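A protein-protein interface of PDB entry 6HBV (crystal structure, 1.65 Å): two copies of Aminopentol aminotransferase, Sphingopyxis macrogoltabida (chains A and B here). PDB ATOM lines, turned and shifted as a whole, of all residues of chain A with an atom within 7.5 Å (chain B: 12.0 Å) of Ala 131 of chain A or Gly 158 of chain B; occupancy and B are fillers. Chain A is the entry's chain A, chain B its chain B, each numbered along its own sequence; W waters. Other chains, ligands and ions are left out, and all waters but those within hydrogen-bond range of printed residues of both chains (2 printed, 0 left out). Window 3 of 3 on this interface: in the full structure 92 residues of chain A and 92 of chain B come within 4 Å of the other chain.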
ATOM      1  N   SER A 123      12.008 -17.046 -12.963  1.00  0.00           N
ATOM      2  CA  SER A 123      11.594 -16.283 -11.795  1.00  0.00           C
ATOM      3  C   SER A 123      12.502 -15.066 -11.624  1.00  0.00           C
ATOM      4  O   SER A 123      12.016 -13.971 -11.318  1.00  0.00           O
ATOM      5  CB  SER A 123      11.566 -17.117 -10.545  1.00  0.00           C
ATOM      6  OG  SER A 123      11.094 -16.343  -9.444  1.00  0.00           O
ATOM      7  N   ALA A 125      14.100 -13.569 -14.071  1.00  0.00           N
ATOM      8  CA  ALA A 125      13.653 -12.659 -15.144  1.00  0.00           C
ATOM      9  C   ALA A 125      12.432 -11.812 -14.743  1.00  0.00           C
ATOM     10  O   ALA A 125      12.377 -10.587 -15.012  1.00  0.00           O
ATOM     11  CB  ALA A 125      13.362 -13.442 -16.402  1.00  0.00           C
ATOM     12  N   MET A 126      11.458 -12.453 -14.110  1.00  0.00           N
ATOM     13  CA  MET A 126      10.199 -11.818 -13.675  1.00  0.00           C
ATOM     14  C   MET A 126      10.505 -10.723 -12.650  1.00  0.00           C
ATOM     15  O   MET A 126      10.046  -9.568 -12.777  1.00  0.00           O
ATOM     16  CB  MET A 126       9.283 -12.867 -13.041  1.00  0.00           C
ATOM     17  CG  MET A 126       8.090 -12.308 -12.303  1.00  0.00           C
ATOM     18  SD  MET A 126       7.091 -13.614 -11.604  1.00  0.00           S
ATOM     19  CE  MET A 126       7.953 -13.855 -10.047  1.00  0.00           C
ATOM     20  N   VAL A 127      11.289 -11.082 -11.619  1.00  0.00           N
ATOM     21  CA  VAL A 127      11.616 -10.141 -10.577  1.00  0.00           C
ATOM     22  C   VAL A 127      12.470  -8.986 -11.163  1.00  0.00           C
ATOM     23  O   VAL A 127      12.248  -7.810 -10.821  1.00  0.00           O
ATOM     24  CB  VAL A 127      12.310 -10.849  -9.402  1.00  0.00           C
ATOM     25  CG1 VAL A 127      12.858  -9.865  -8.398  1.00  0.00           C
ATOM     26  CG2 VAL A 127      11.398 -11.851  -8.738  1.00  0.00           C
ATOM     27  N   LEU A 128      13.430  -9.317 -12.028  1.00  0.00           N
ATOM     28  CA  LEU A 128      14.297  -8.349 -12.663  1.00  0.00           C
ATOM     29  C   LEU A 128      13.418  -7.333 -13.416  1.00  0.00           C
ATOM     30  O   LEU A 128      13.607  -6.112 -13.269  1.00  0.00           O
ATOM     31  CB  LEU A 128      15.268  -9.028 -13.619  1.00  0.00           C
ATOM     32  CG  LEU A 128      16.411  -8.169 -14.144  1.00  0.00           C
ATOM     33  CD1 LEU A 128      17.515  -9.057 -14.728  1.00  0.00           C
ATOM     34  CD2 LEU A 128      15.951  -7.173 -15.223  1.00  0.00           C
ATOM     35  N   ALA A 129      12.464  -7.824 -14.216  1.00  0.00           N
ATOM     36  CA  ALA A 129      11.658  -6.907 -15.029  1.00  0.00           C
ATOM     37  C   ALA A 129      10.808  -5.945 -14.174  1.00  0.00           C
ATOM     38  O   ALA A 129      10.624  -4.780 -14.552  1.00  0.00           O
ATOM     39  CB  ALA A 129      10.782  -7.704 -15.949  1.00  0.00           C
ATOM     40  N   ARG A 130      10.286  -6.420 -13.040  1.00  0.00           N
ATOM     41  CA  ARG A 130       9.528  -5.604 -12.115  1.00  0.00           C
ATOM     42  C   ARG A 130      10.447  -4.523 -11.530  1.00  0.00           C
ATOM     43  O   ARG A 130      10.060  -3.344 -11.450  1.00  0.00           O
ATOM     44  CB  ARG A 130       8.857  -6.480 -11.056  1.00  0.00           C
ATOM     45  CG  ARG A 130       7.686  -7.277 -11.600  1.00  0.00           C
ATOM     46  CD  ARG A 130       7.052  -8.225 -10.637  1.00  0.00           C
ATOM     47  NE  ARG A 130       5.795  -8.704 -11.182  1.00  0.00           N
ATOM     48  CZ  ARG A 130       5.136  -9.767 -10.754  1.00  0.00           C
ATOM     49  NH1 ARG A 130       5.682 -10.548  -9.817  1.00  0.00           N
ATOM     50  NH2 ARG A 130       3.937 -10.027 -11.280  1.00  0.00           N
ATOM     51  N   ALA A 131      11.666  -4.915 -11.119  1.00  0.00           N
ATOM     52  CA  ALA A 131      12.622  -3.956 -10.569  1.00  0.00           C
ATOM     53  C   ALA A 131      13.039  -2.920 -11.628  1.00  0.00           C
ATOM     54  O   ALA A 131      13.191  -1.750 -11.323  1.00  0.00           O
ATOM     55  CB  ALA A 131      13.832  -4.668 -10.028  1.00  0.00           C
ATOM     56  N   HIS A 132      13.225  -3.364 -12.863  1.00  0.00           N
ATOM     57  CA  HIS A 132      13.716  -2.536 -13.927  1.00  0.00           C
ATOM     58  C   HIS A 132      12.681  -1.463 -14.261  1.00  0.00           C
ATOM     59  O   HIS A 132      13.042  -0.304 -14.440  1.00  0.00           O
ATOM     60  CB  HIS A 132      13.976  -3.380 -15.173  1.00  0.00           C
ATOM     61  CG  HIS A 132      14.355  -2.592 -16.372  1.00  0.00           C
ATOM     62  ND1 HIS A 132      15.639  -2.138 -16.585  1.00  0.00           N
ATOM     63  CD2 HIS A 132      13.614  -2.175 -17.423  1.00  0.00           C
ATOM     64  CE1 HIS A 132      15.675  -1.475 -17.717  1.00  0.00           C
ATOM     65  NE2 HIS A 132      14.432  -1.484 -18.258  1.00  0.00           N
ATOM     66  N   THR A 133      11.420  -1.887 -14.343  1.00  0.00           N
ATOM     67  CA  THR A 133      10.349  -1.000 -14.874  1.00  0.00           C
ATOM     68  C   THR A 133       9.605  -0.261 -13.772  1.00  0.00           C
ATOM     69  O   THR A 133       8.931   0.758 -14.046  1.00  0.00           O
ATOM     70  CB  THR A 133       9.320  -1.783 -15.702  1.00  0.00           C
ATOM     71  OG1 THR A 133       8.736  -2.757 -14.850  1.00  0.00           O
ATOM     72  CG2 THR A 133       9.886  -2.442 -16.931  1.00  0.00           C
ATOM     73  N   GLY A 134       9.695  -0.749 -12.533  1.00  0.00           N
ATOM     74  CA  GLY A 134       8.797  -0.359 -11.443  1.00  0.00           C
ATOM     75  C   GLY A 134       7.310  -0.637 -11.691  1.00  0.00           C
ATOM     76  O   GLY A 134       6.472   0.008 -11.075  1.00  0.00           O
ATOM     77  N   ARG A 135       6.980  -1.586 -12.576  1.00  0.00           N
ATOM     78  CA  ARG A 135       5.595  -1.976 -12.923  1.00  0.00           C
ATOM     79  C   ARG A 135       5.333  -3.406 -12.475  1.00  0.00           C
ATOM     80  O   ARG A 135       6.278  -4.112 -12.117  1.00  0.00           O
ATOM     81  CB  ARG A 135       5.399  -1.924 -14.428  1.00  0.00           C
ATOM     82  CG  ARG A 135       5.587  -0.521 -14.966  1.00  0.00           C
ATOM     83  CD  ARG A 135       5.665  -0.600 -16.465  1.00  0.00           C
ATOM     84  NE  ARG A 135       6.260   0.594 -17.008  1.00  0.00           N
ATOM     85  CZ  ARG A 135       6.735   0.698 -18.234  1.00  0.00           C
ATOM     86  NH1 ARG A 135       7.241   1.853 -18.625  1.00  0.00           N
ATOM     87  NH2 ARG A 135       6.708  -0.324 -19.068  1.00  0.00           N
ATOM     88  N   LYS A 136       4.069  -3.817 -12.501  1.00  0.00           N
ATOM     89  CA  LYS A 136       3.686  -5.063 -11.882  1.00  0.00           C
ATOM     90  C   LYS A 136       3.400  -6.179 -12.893  1.00  0.00           C
ATOM     91  O   LYS A 136       3.677  -7.352 -12.596  1.00  0.00           O
ATOM     92  CB  LYS A 136       2.437  -4.849 -11.031  1.00  0.00           C
ATOM     93  CG  LYS A 136       2.639  -3.920  -9.857  1.00  0.00           C
ATOM     94  CD  LYS A 136       1.423  -3.752  -9.039  1.00  0.00           C
ATOM     95  CE  LYS A 136       1.684  -2.813  -7.887  1.00  0.00           C
ATOM     96  NZ  LYS A 136       0.448  -2.661  -7.084  1.00  0.00           N
ATOM     97  N   ALA A 190       5.598  -4.846 -17.110  1.00  0.00           N
ATOM     98  CA  ALA A 190       6.999  -5.058 -16.747  1.00  0.00           C
ATOM     99  C   ALA A 190       7.709  -5.927 -17.788  1.00  0.00           C
ATOM    100  O   ALA A 190       8.857  -5.669 -18.117  1.00  0.00           O
ATOM    101  CB  ALA A 190       7.054  -5.728 -15.397  1.00  0.00           C
ATOM    102  N   ASP A 277      21.418  -2.975 -14.428  1.00  0.00           N
ATOM    103  CA  ASP A 277      21.268  -2.328 -13.132  1.00  0.00           C
ATOM    104  C   ASP A 277      20.233  -3.070 -12.294  1.00  0.00           C
ATOM    105  O   ASP A 277      20.461  -3.308 -11.079  1.00  0.00           O
ATOM    106  CB  ASP A 277      20.871  -0.850 -13.261  1.00  0.00           C
ATOM    107  CG  ASP A 277      22.014   0.054 -13.705  1.00  0.00           C
ATOM    108  OD1 ASP A 277      23.182  -0.292 -13.471  1.00  0.00           O
ATOM    109  OD2 ASP A 277      21.718   1.108 -14.291  1.00  0.00           O
ATOM    110  N   ALA A 278      19.106  -3.430 -12.933  1.00  0.00           N
ATOM    111  CA  ALA A 278      18.054  -4.150 -12.221  1.00  0.00           C
ATOM    112  C   ALA A 278      18.578  -5.533 -11.787  1.00  0.00           C
ATOM    113  O   ALA A 278      18.268  -5.992 -10.724  1.00  0.00           O
ATOM    114  CB  ALA A 278      16.816  -4.281 -13.074  1.00  0.00           C
ATOM    115  N   ALA A 279      19.363  -6.161 -12.636  1.00  0.00           N
ATOM    116  CA  ALA A 279      19.966  -7.456 -12.292  1.00  0.00           C
ATOM    117  C   ALA A 279      20.841  -7.332 -11.037  1.00  0.00           C
ATOM    118  O   ALA A 279      20.898  -8.282 -10.244  1.00  0.00           O
ATOM    119  CB  ALA A 279      20.759  -7.963 -13.449  1.00  0.00           C
ATOM    120  N   ASP A 281      20.306  -5.105  -8.604  1.00  0.00           N
ATOM    121  CA  ASP A 281      19.470  -4.615  -7.507  1.00  0.00           C
ATOM    122  C   ASP A 281      18.688  -5.754  -6.857  1.00  0.00           C
ATOM    123  O   ASP A 281      18.446  -5.729  -5.674  1.00  0.00           O
ATOM    124  CB  ASP A 281      18.467  -3.550  -7.960  1.00  0.00           C
ATOM    125  CG  ASP A 281      19.068  -2.164  -8.194  1.00  0.00           C
ATOM    126  OD1 ASP A 281      20.235  -1.919  -7.753  1.00  0.00           O
ATOM    127  OD2 ASP A 281      18.364  -1.323  -8.827  1.00  0.00           O
ATOM    128  N   ILE A 282      18.299  -6.751  -7.651  1.00  0.00           N
ATOM    129  CA  ILE A 282      17.526  -7.833  -7.101  1.00  0.00           C
ATOM    130  C   ILE A 282      18.440  -8.746  -6.279  1.00  0.00           C
ATOM    131  O   ILE A 282      19.646  -8.757  -6.440  1.00  0.00           O
ATOM    132  CB  ILE A 282      16.777  -8.607  -8.199  1.00  0.00           C
ATOM    133  CG1 ILE A 282      17.737  -9.340  -9.134  1.00  0.00           C
ATOM    134  CG2 ILE A 282      15.871  -7.655  -8.951  1.00  0.00           C
ATOM    135  CD1 ILE A 282      17.076 -10.191 -10.193  1.00  0.00           C
ATOM    136  N   PHE A 283      17.825  -9.513  -5.393  1.00  0.00           N
ATOM    137  CA  PHE A 283      18.578 -10.521  -4.619  1.00  0.00           C
ATOM    138  C   PHE A 283      18.085 -11.931  -4.969  1.00  0.00           C
ATOM    139  O   PHE A 283      16.966 -12.326  -4.593  1.00  0.00           O
ATOM    140  CB  PHE A 283      18.443 -10.345  -3.108  1.00  0.00           C
ATOM    141  CG  PHE A 283      19.338 -11.316  -2.394  1.00  0.00           C
ATOM    142  CD1 PHE A 283      20.702 -11.094  -2.369  1.00  0.00           C
ATOM    143  CD2 PHE A 283      18.819 -12.443  -1.762  1.00  0.00           C
ATOM    144  CE1 PHE A 283      21.559 -11.973  -1.722  1.00  0.00           C
ATOM    145  CE2 PHE A 283      19.671 -13.321  -1.114  1.00  0.00           C
ATOM    146  CZ  PHE A 283      21.035 -13.080  -1.099  1.00  0.00           C
ATOM    147  N   PRO B  19      26.530  -9.333 -13.769  1.00  0.00           N
ATOM    148  CA  PRO B  19      26.105  -8.082 -13.154  1.00  0.00           C
ATOM    149  C   PRO B  19      26.801  -7.862 -11.807  1.00  0.00           C
ATOM    150  O   PRO B  19      26.677  -8.706 -10.900  1.00  0.00           O
ATOM    151  CB  PRO B  19      24.606  -8.262 -12.949  1.00  0.00           C
ATOM    152  CG  PRO B  19      24.252  -9.322 -13.948  1.00  0.00           C
ATOM    153  CD  PRO B  19      25.431 -10.270 -13.996  1.00  0.00           C
ATOM    154  N   ALA B 148      15.391 -17.452  -1.456  1.00  0.00           N
ATOM    155  CA  ALA B 148      15.390 -16.215  -2.165  1.00  0.00           C
ATOM    156  C   ALA B 148      14.313 -16.204  -3.260  1.00  0.00           C
ATOM    157  O   ALA B 148      14.492 -15.663  -4.328  1.00  0.00           O
ATOM    158  CB  ALA B 148      16.795 -15.930  -2.658  1.00  0.00           C
ATOM    159  N   SER B 149      13.168 -16.816  -2.962  1.00  0.00           N
ATOM    160  CA  SER B 149      11.971 -16.783  -3.830  1.00  0.00           C
ATOM    161  C   SER B 149      11.222 -15.473  -3.591  1.00  0.00           C
ATOM    162  O   SER B 149      11.471 -14.780  -2.626  1.00  0.00           O
ATOM    163  CB  SER B 149      11.057 -17.981  -3.538  1.00  0.00           C
ATOM    164  OG  SER B 149      11.815 -19.181  -3.532  1.00  0.00           O
ATOM    165  N   PRO B 150      10.276 -15.071  -4.455  1.00  0.00           N
ATOM    166  CA  PRO B 150       9.475 -13.880  -4.146  1.00  0.00           C
ATOM    167  C   PRO B 150       8.800 -13.853  -2.762  1.00  0.00           C
ATOM    168  O   PRO B 150       8.709 -12.792  -2.132  1.00  0.00           O
ATOM    169  CB  PRO B 150       8.515 -13.828  -5.352  1.00  0.00           C
ATOM    170  CG  PRO B 150       9.288 -14.530  -6.453  1.00  0.00           C
ATOM    171  CD  PRO B 150       9.937 -15.708  -5.739  1.00  0.00           C
ATOM    172  N   TRP B 151       8.325 -14.993  -2.261  1.00  0.00           N
ATOM    173  CA  TRP B 151       7.609 -14.994  -1.015  1.00  0.00           C
ATOM    174  C   TRP B 151       8.553 -14.779   0.180  1.00  0.00           C
ATOM    175  O   TRP B 151       8.081 -14.380   1.253  1.00  0.00           O
ATOM    176  CB  TRP B 151       6.806 -16.306  -0.844  1.00  0.00           C
ATOM    177  CG  TRP B 151       7.552 -17.579  -0.548  1.00  0.00           C
ATOM    178  CD1 TRP B 151       8.134 -18.433  -1.445  1.00  0.00           C
ATOM    179  CD2 TRP B 151       7.786 -18.165   0.750  1.00  0.00           C
ATOM    180  NE1 TRP B 151       8.707 -19.488  -0.798  1.00  0.00           N
ATOM    181  CE2 TRP B 151       8.514 -19.361   0.545  1.00  0.00           C
ATOM    182  CE3 TRP B 151       7.456 -17.801   2.057  1.00  0.00           C
ATOM    183  CZ2 TRP B 151       8.915 -20.187   1.600  1.00  0.00           C
ATOM    184  CZ3 TRP B 151       7.848 -18.617   3.106  1.00  0.00           C
ATOM    185  CH2 TRP B 151       8.571 -19.796   2.873  1.00  0.00           C
ATOM    186  N   ASN B 152       9.864 -15.042   0.020  1.00  0.00           N
ATOM    187  CA  ASN B 152      10.732 -15.056   1.227  1.00  0.00           C
ATOM    188  C   ASN B 152      12.037 -14.261   1.083  1.00  0.00           C
ATOM    189  O   ASN B 152      12.702 -14.048   2.112  1.00  0.00           O
ATOM    190  CB  ASN B 152      10.994 -16.487   1.728  1.00  0.00           C
ATOM    191  CG  ASN B 152      11.587 -17.378   0.661  1.00  0.00           C
ATOM    192  OD1 ASN B 152      12.051 -16.882  -0.376  1.00  0.00           O
ATOM    193  ND2 ASN B 152      11.578 -18.677   0.902  1.00  0.00           N
ATOM    194  N   THR B 153      12.429 -13.814  -0.120  1.00  0.00           N
ATOM    195  CA  THR B 153      13.716 -13.162  -0.313  1.00  0.00           C
ATOM    196  C   THR B 153      13.828 -11.990   0.657  1.00  0.00           C
ATOM    197  O   THR B 153      12.877 -11.212   0.819  1.00  0.00           O
ATOM    198  CB  THR B 153      13.942 -12.775  -1.781  1.00  0.00           C
ATOM    199  OG1 THR B 153      15.298 -12.335  -1.899  1.00  0.00           O
ATOM    200  CG2 THR B 153      12.970 -11.729  -2.277  1.00  0.00           C
ATOM    201  N   PRO B 154      14.993 -11.840   1.326  1.00  0.00           N
ATOM    202  CA  PRO B 154      15.204 -10.744   2.269  1.00  0.00           C
ATOM    203  C   PRO B 154      15.322  -9.335   1.672  1.00  0.00           C
ATOM    204  O   PRO B 154      15.090  -8.366   2.400  1.00  0.00           O
ATOM    205  CB  PRO B 154      16.515 -11.131   2.980  1.00  0.00           C
ATOM    206  CG  PRO B 154      17.256 -11.935   1.935  1.00  0.00           C
ATOM    207  CD  PRO B 154      16.168 -12.720   1.219  1.00  0.00           C
ATOM    208  N   HIS B 155      15.672  -9.217   0.391  1.00  0.00           N
ATOM    209  CA  HIS B 155      15.742  -7.912  -0.233  1.00  0.00           C
ATOM    210  C   HIS B 155      14.698  -7.849  -1.348  1.00  0.00           C
ATOM    211  O   HIS B 155      14.674  -8.727  -2.192  1.00  0.00           O
ATOM    212  CB  HIS B 155      17.165  -7.603  -0.744  1.00  0.00           C
ATOM    213  CG  HIS B 155      17.225  -6.342  -1.554  1.00  0.00           C
ATOM    214  ND1 HIS B 155      17.442  -5.094  -0.969  1.00  0.00           N
ATOM    215  CD2 HIS B 155      17.092  -6.120  -2.891  1.00  0.00           C
ATOM    216  CE1 HIS B 155      17.442  -4.161  -1.909  1.00  0.00           C
ATOM    217  NE2 HIS B 155      17.229  -4.767  -3.104  1.00  0.00           N
ATOM    218  N   THR B 156      13.855  -6.807  -1.327  1.00  0.00           N
ATOM    219  CA  THR B 156      12.587  -6.877  -2.022  1.00  0.00           C
ATOM    220  C   THR B 156      12.546  -6.043  -3.316  1.00  0.00           C
ATOM    221  O   THR B 156      11.439  -5.734  -3.767  1.00  0.00           O
ATOM    222  CB  THR B 156      11.475  -6.515  -1.039  1.00  0.00           C
ATOM    223  OG1 THR B 156      11.734  -5.191  -0.574  1.00  0.00           O
ATOM    224  CG2 THR B 156      11.425  -7.474   0.129  1.00  0.00           C
ATOM    225  N   ALA B 157      13.691  -5.678  -3.914  1.00  0.00           N
ATOM    226  CA  ALA B 157      13.650  -5.069  -5.252  1.00  0.00           C
ATOM    227  C   ALA B 157      12.940  -6.051  -6.195  1.00  0.00           C
ATOM    228  O   ALA B 157      13.281  -7.215  -6.245  1.00  0.00           O
ATOM    229  CB  ALA B 157      15.033  -4.675  -5.764  1.00  0.00           C
ATOM    230  N   GLY B 158      11.937  -5.555  -6.933  1.00  0.00           N
ATOM    231  CA  GLY B 158      11.216  -6.370  -7.885  1.00  0.00           C
ATOM    232  C   GLY B 158      10.171  -7.292  -7.285  1.00  0.00           C
ATOM    233  O   GLY B 158       9.536  -8.071  -8.015  1.00  0.00           O
ATOM    234  N   ILE B 159       9.969  -7.221  -5.964  1.00  0.00           N
ATOM    235  CA  ILE B 159       9.027  -8.056  -5.260  1.00  0.00           C
ATOM    236  C   ILE B 159       7.763  -7.253  -4.975  1.00  0.00           C
ATOM    237  O   ILE B 159       7.851  -6.106  -4.536  1.00  0.00           O
ATOM    238  CB  ILE B 159       9.631  -8.594  -3.950  1.00  0.00           C
ATOM    239  CG1 ILE B 159      10.951  -9.344  -4.181  1.00  0.00           C
ATOM    240  CG2 ILE B 159       8.615  -9.414  -3.182  1.00  0.00           C
ATOM    241  CD1 ILE B 159      10.859 -10.437  -5.221  1.00  0.00           C
ATOM    242  N   LEU B 160       6.602  -7.867  -5.217  1.00  0.00           N
ATOM    243  CA  LEU B 160       5.316  -7.194  -5.017  1.00  0.00           C
ATOM    244  C   LEU B 160       4.731  -7.543  -3.648  1.00  0.00           C
ATOM    245  O   LEU B 160       4.981  -8.654  -3.109  1.00  0.00           O
ATOM    246  CB  LEU B 160       4.337  -7.638  -6.098  1.00  0.00           C
ATOM    247  CG  LEU B 160       4.798  -7.428  -7.538  1.00  0.00           C
ATOM    248  CD1 LEU B 160       3.648  -7.719  -8.487  1.00  0.00           C
ATOM    249  CD2 LEU B 160       5.329  -6.011  -7.756  1.00  0.00           C
ATOM    250  N   ALA B 161       3.937  -6.616  -3.078  1.00  0.00           N
ATOM    251  CA  ALA B 161       3.262  -6.926  -1.794  1.00  0.00           C
ATOM    252  C   ALA B 161       2.469  -8.242  -1.916  1.00  0.00           C
ATOM    253  O   ALA B 161       2.426  -9.012  -0.991  1.00  0.00           O
ATOM    254  CB  ALA B 161       2.382  -5.768  -1.356  1.00  0.00           C
ATOM    255  N   SER B 162       1.855  -8.470  -3.089  1.00  0.00           N
ATOM    256  CA  SER B 162       1.022  -9.633  -3.374  1.00  0.00           C
ATOM    257  C   SER B 162       1.825 -10.945  -3.341  1.00  0.00           C
ATOM    258  O   SER B 162       1.238 -12.002  -3.140  1.00  0.00           O
ATOM    259  CB  SER B 162       0.288  -9.490  -4.697  1.00  0.00           C
ATOM    260  OG  SER B 162       1.159  -9.242  -5.758  1.00  0.00           O
ATOM    261  N   ASP B 163       3.140 -10.863  -3.532  1.00  0.00           N
ATOM    262  CA  ASP B 163       4.035 -12.055  -3.494  1.00  0.00           C
ATOM    263  C   ASP B 163       4.069 -12.679  -2.088  1.00  0.00           C
ATOM    264  O   ASP B 163       4.314 -13.867  -1.935  1.00  0.00           O
ATOM    265  CB  ASP B 163       5.433 -11.640  -3.964  1.00  0.00           C
ATOM    266  CG  ASP B 163       5.520 -11.414  -5.455  1.00  0.00           C
ATOM    267  OD1 ASP B 163       4.686 -11.965  -6.177  1.00  0.00           O
ATOM    268  OD2 ASP B 163       6.411 -10.700  -5.877  1.00  0.00           O
ATOM    269  N   ARG B 164       3.828 -11.864  -1.049  1.00  0.00           N
ATOM    270  CA  ARG B 164       3.930 -12.328   0.317  1.00  0.00           C
ATOM    271  C   ARG B 164       2.780 -11.794   1.189  1.00  0.00           C
ATOM    272  O   ARG B 164       2.905 -11.721   2.394  1.00  0.00           O
ATOM    273  CB  ARG B 164       5.301 -11.928   0.859  1.00  0.00           C
ATOM    274  CG  ARG B 164       5.548 -10.429   0.796  1.00  0.00           C
ATOM    275  CD  ARG B 164       6.994 -10.094   0.988  1.00  0.00           C
ATOM    276  NE  ARG B 164       7.979 -10.855   0.211  1.00  0.00           N
ATOM    277  CZ  ARG B 164       9.246 -10.873   0.570  1.00  0.00           C
ATOM    278  NH1 ARG B 164       9.599 -10.212   1.663  1.00  0.00           N
ATOM    279  NH2 ARG B 164      10.145 -11.532  -0.129  1.00  0.00           N
HETATM  280  O   HOH W   1      14.938  -8.954  -4.851  1.00  0.00           O
HETATM  281  O   HOH W   2       7.874 -10.344  -8.077  1.00  0.00           O
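Water W2 lies within hydrogen-bond range of the side-chain carboxylate of Asp 163 of chain B, the guanidinium group of Arg 130 of chain A and the backbone carbonyl oxygen of Gly 158 of chain B.
Water W1 lies within hydrogen-bond range of the backbone carbonyl oxygen of His 155 of chain B, the backbone carbonyl oxygen of Ala 157 of chain B and the backbone NH of Phe 283 of chain A.
NE of Arg 130 of chain A sits at hydrogen-bond distance from O of Lys 136 of chain A.
NH2 of Arg 164 of chain B lies within hydrogen-bond range of O of Pro 150 of chain B.
The backbone carbonyl oxygen (O) of Thr 153 of chain B sits at hydrogen-bond distance from the guanidinium group (NH2) of Arg 164 of chain B, at 2.9 Å.
The side-chain carboxylate of Asp 163 of chain B lies within hydrogen-bond range of the backbone NH of Leu 160 of chain B (2.9 Å).
Of the 18 printed residues of chain B, 9 touch a printed residue of chain A.
Hydrophobic or aromatic side chains of chain A that line the printed part of chain B: Met 126, Val 127, Ala 131, Ala 279, Ile 282 and Phe 283.
Among the printed residues, 15 pairs touch across the chains.
Of the printed residues of chain B, Ala 131 of chain A touches Gly 158 (3.6 Å).
Of chain A, only Val 127, Arg 130 and Ala 131 come within 4 Å of Gly 158 of chain B.
Of chain B, only Ala 157 (3.4 Å), Gly 158 (3.4 Å) and Ile 159 (3.8 Å) come within 4 Å of Val 127 of chain A.
No residue of chain B comes within 4 Å of Leu 128 of chain A.
No residue of chain B comes within 4 Å of Ala 129 of chain A.
No residue of chain B comes within 4 Å of Thr 133 of chain A.
No residue of chain B comes within 4 Å of Gly 134 of chain A.
No residue of chain B comes within 4 Å of Ala 278 of chain A.
Of the printed residues of chain A, Pro 154 of chain B touches Phe 283 (3.999 Å).
Of the printed residues of chain A, Ile 159 of chain B touches Val 127.
Ala 190 of chain A touches none of the printed residues of chain B.
The nearest residue of chain B that does not touch Ala 131 of chain A is Ala 157 of chain B (4.2 Å).
Ser 123 of chain A touches Pro 150 of chain B.
O of Ala 157 of chain B touches CG1 of Val 127 of chain A (3.4 Å).
Gly 158 of chain B touches Val 127 of chain A.
Gly 158 of chain B touches Arg 130 of chain A (O to CB, 3.5 Å).
CZ of Arg 130 of chain A touches CD1 of Leu 160 of chain B (3.4 Å).
Ala 131 of chain A touches Gly 158 of chain B (N to CA, 3.6 Å).
Ala 279 of chain A touches Pro 19 of chain B (CB to CG, 3.8 Å).
Asp 281 of chain A touches Ala 157 of chain B.
Ile 282 of chain A touches Ala 157 of chain B (CG2 to O, 3.8 Å).
CB of Phe 283 of chain A touches CB of His 155 of chain B, 3.8 Å away.
No position is printed for both chains.
Of the 15 pairs that touch across the chains among the printed residues, none has its exchanged pair printed and touching as well.
The backbone carbonyl oxygen of Asp 281 of chain A is in hydrogen-bond range of a ring nitrogen (NE2) of His 155 of chain B (3.0 Å).
The side-chain hydroxyl of Thr 153 of chain B sits at hydrogen-bond distance from the backbone carbonyl oxygen of Phe 283 of chain A (3.2 Å).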
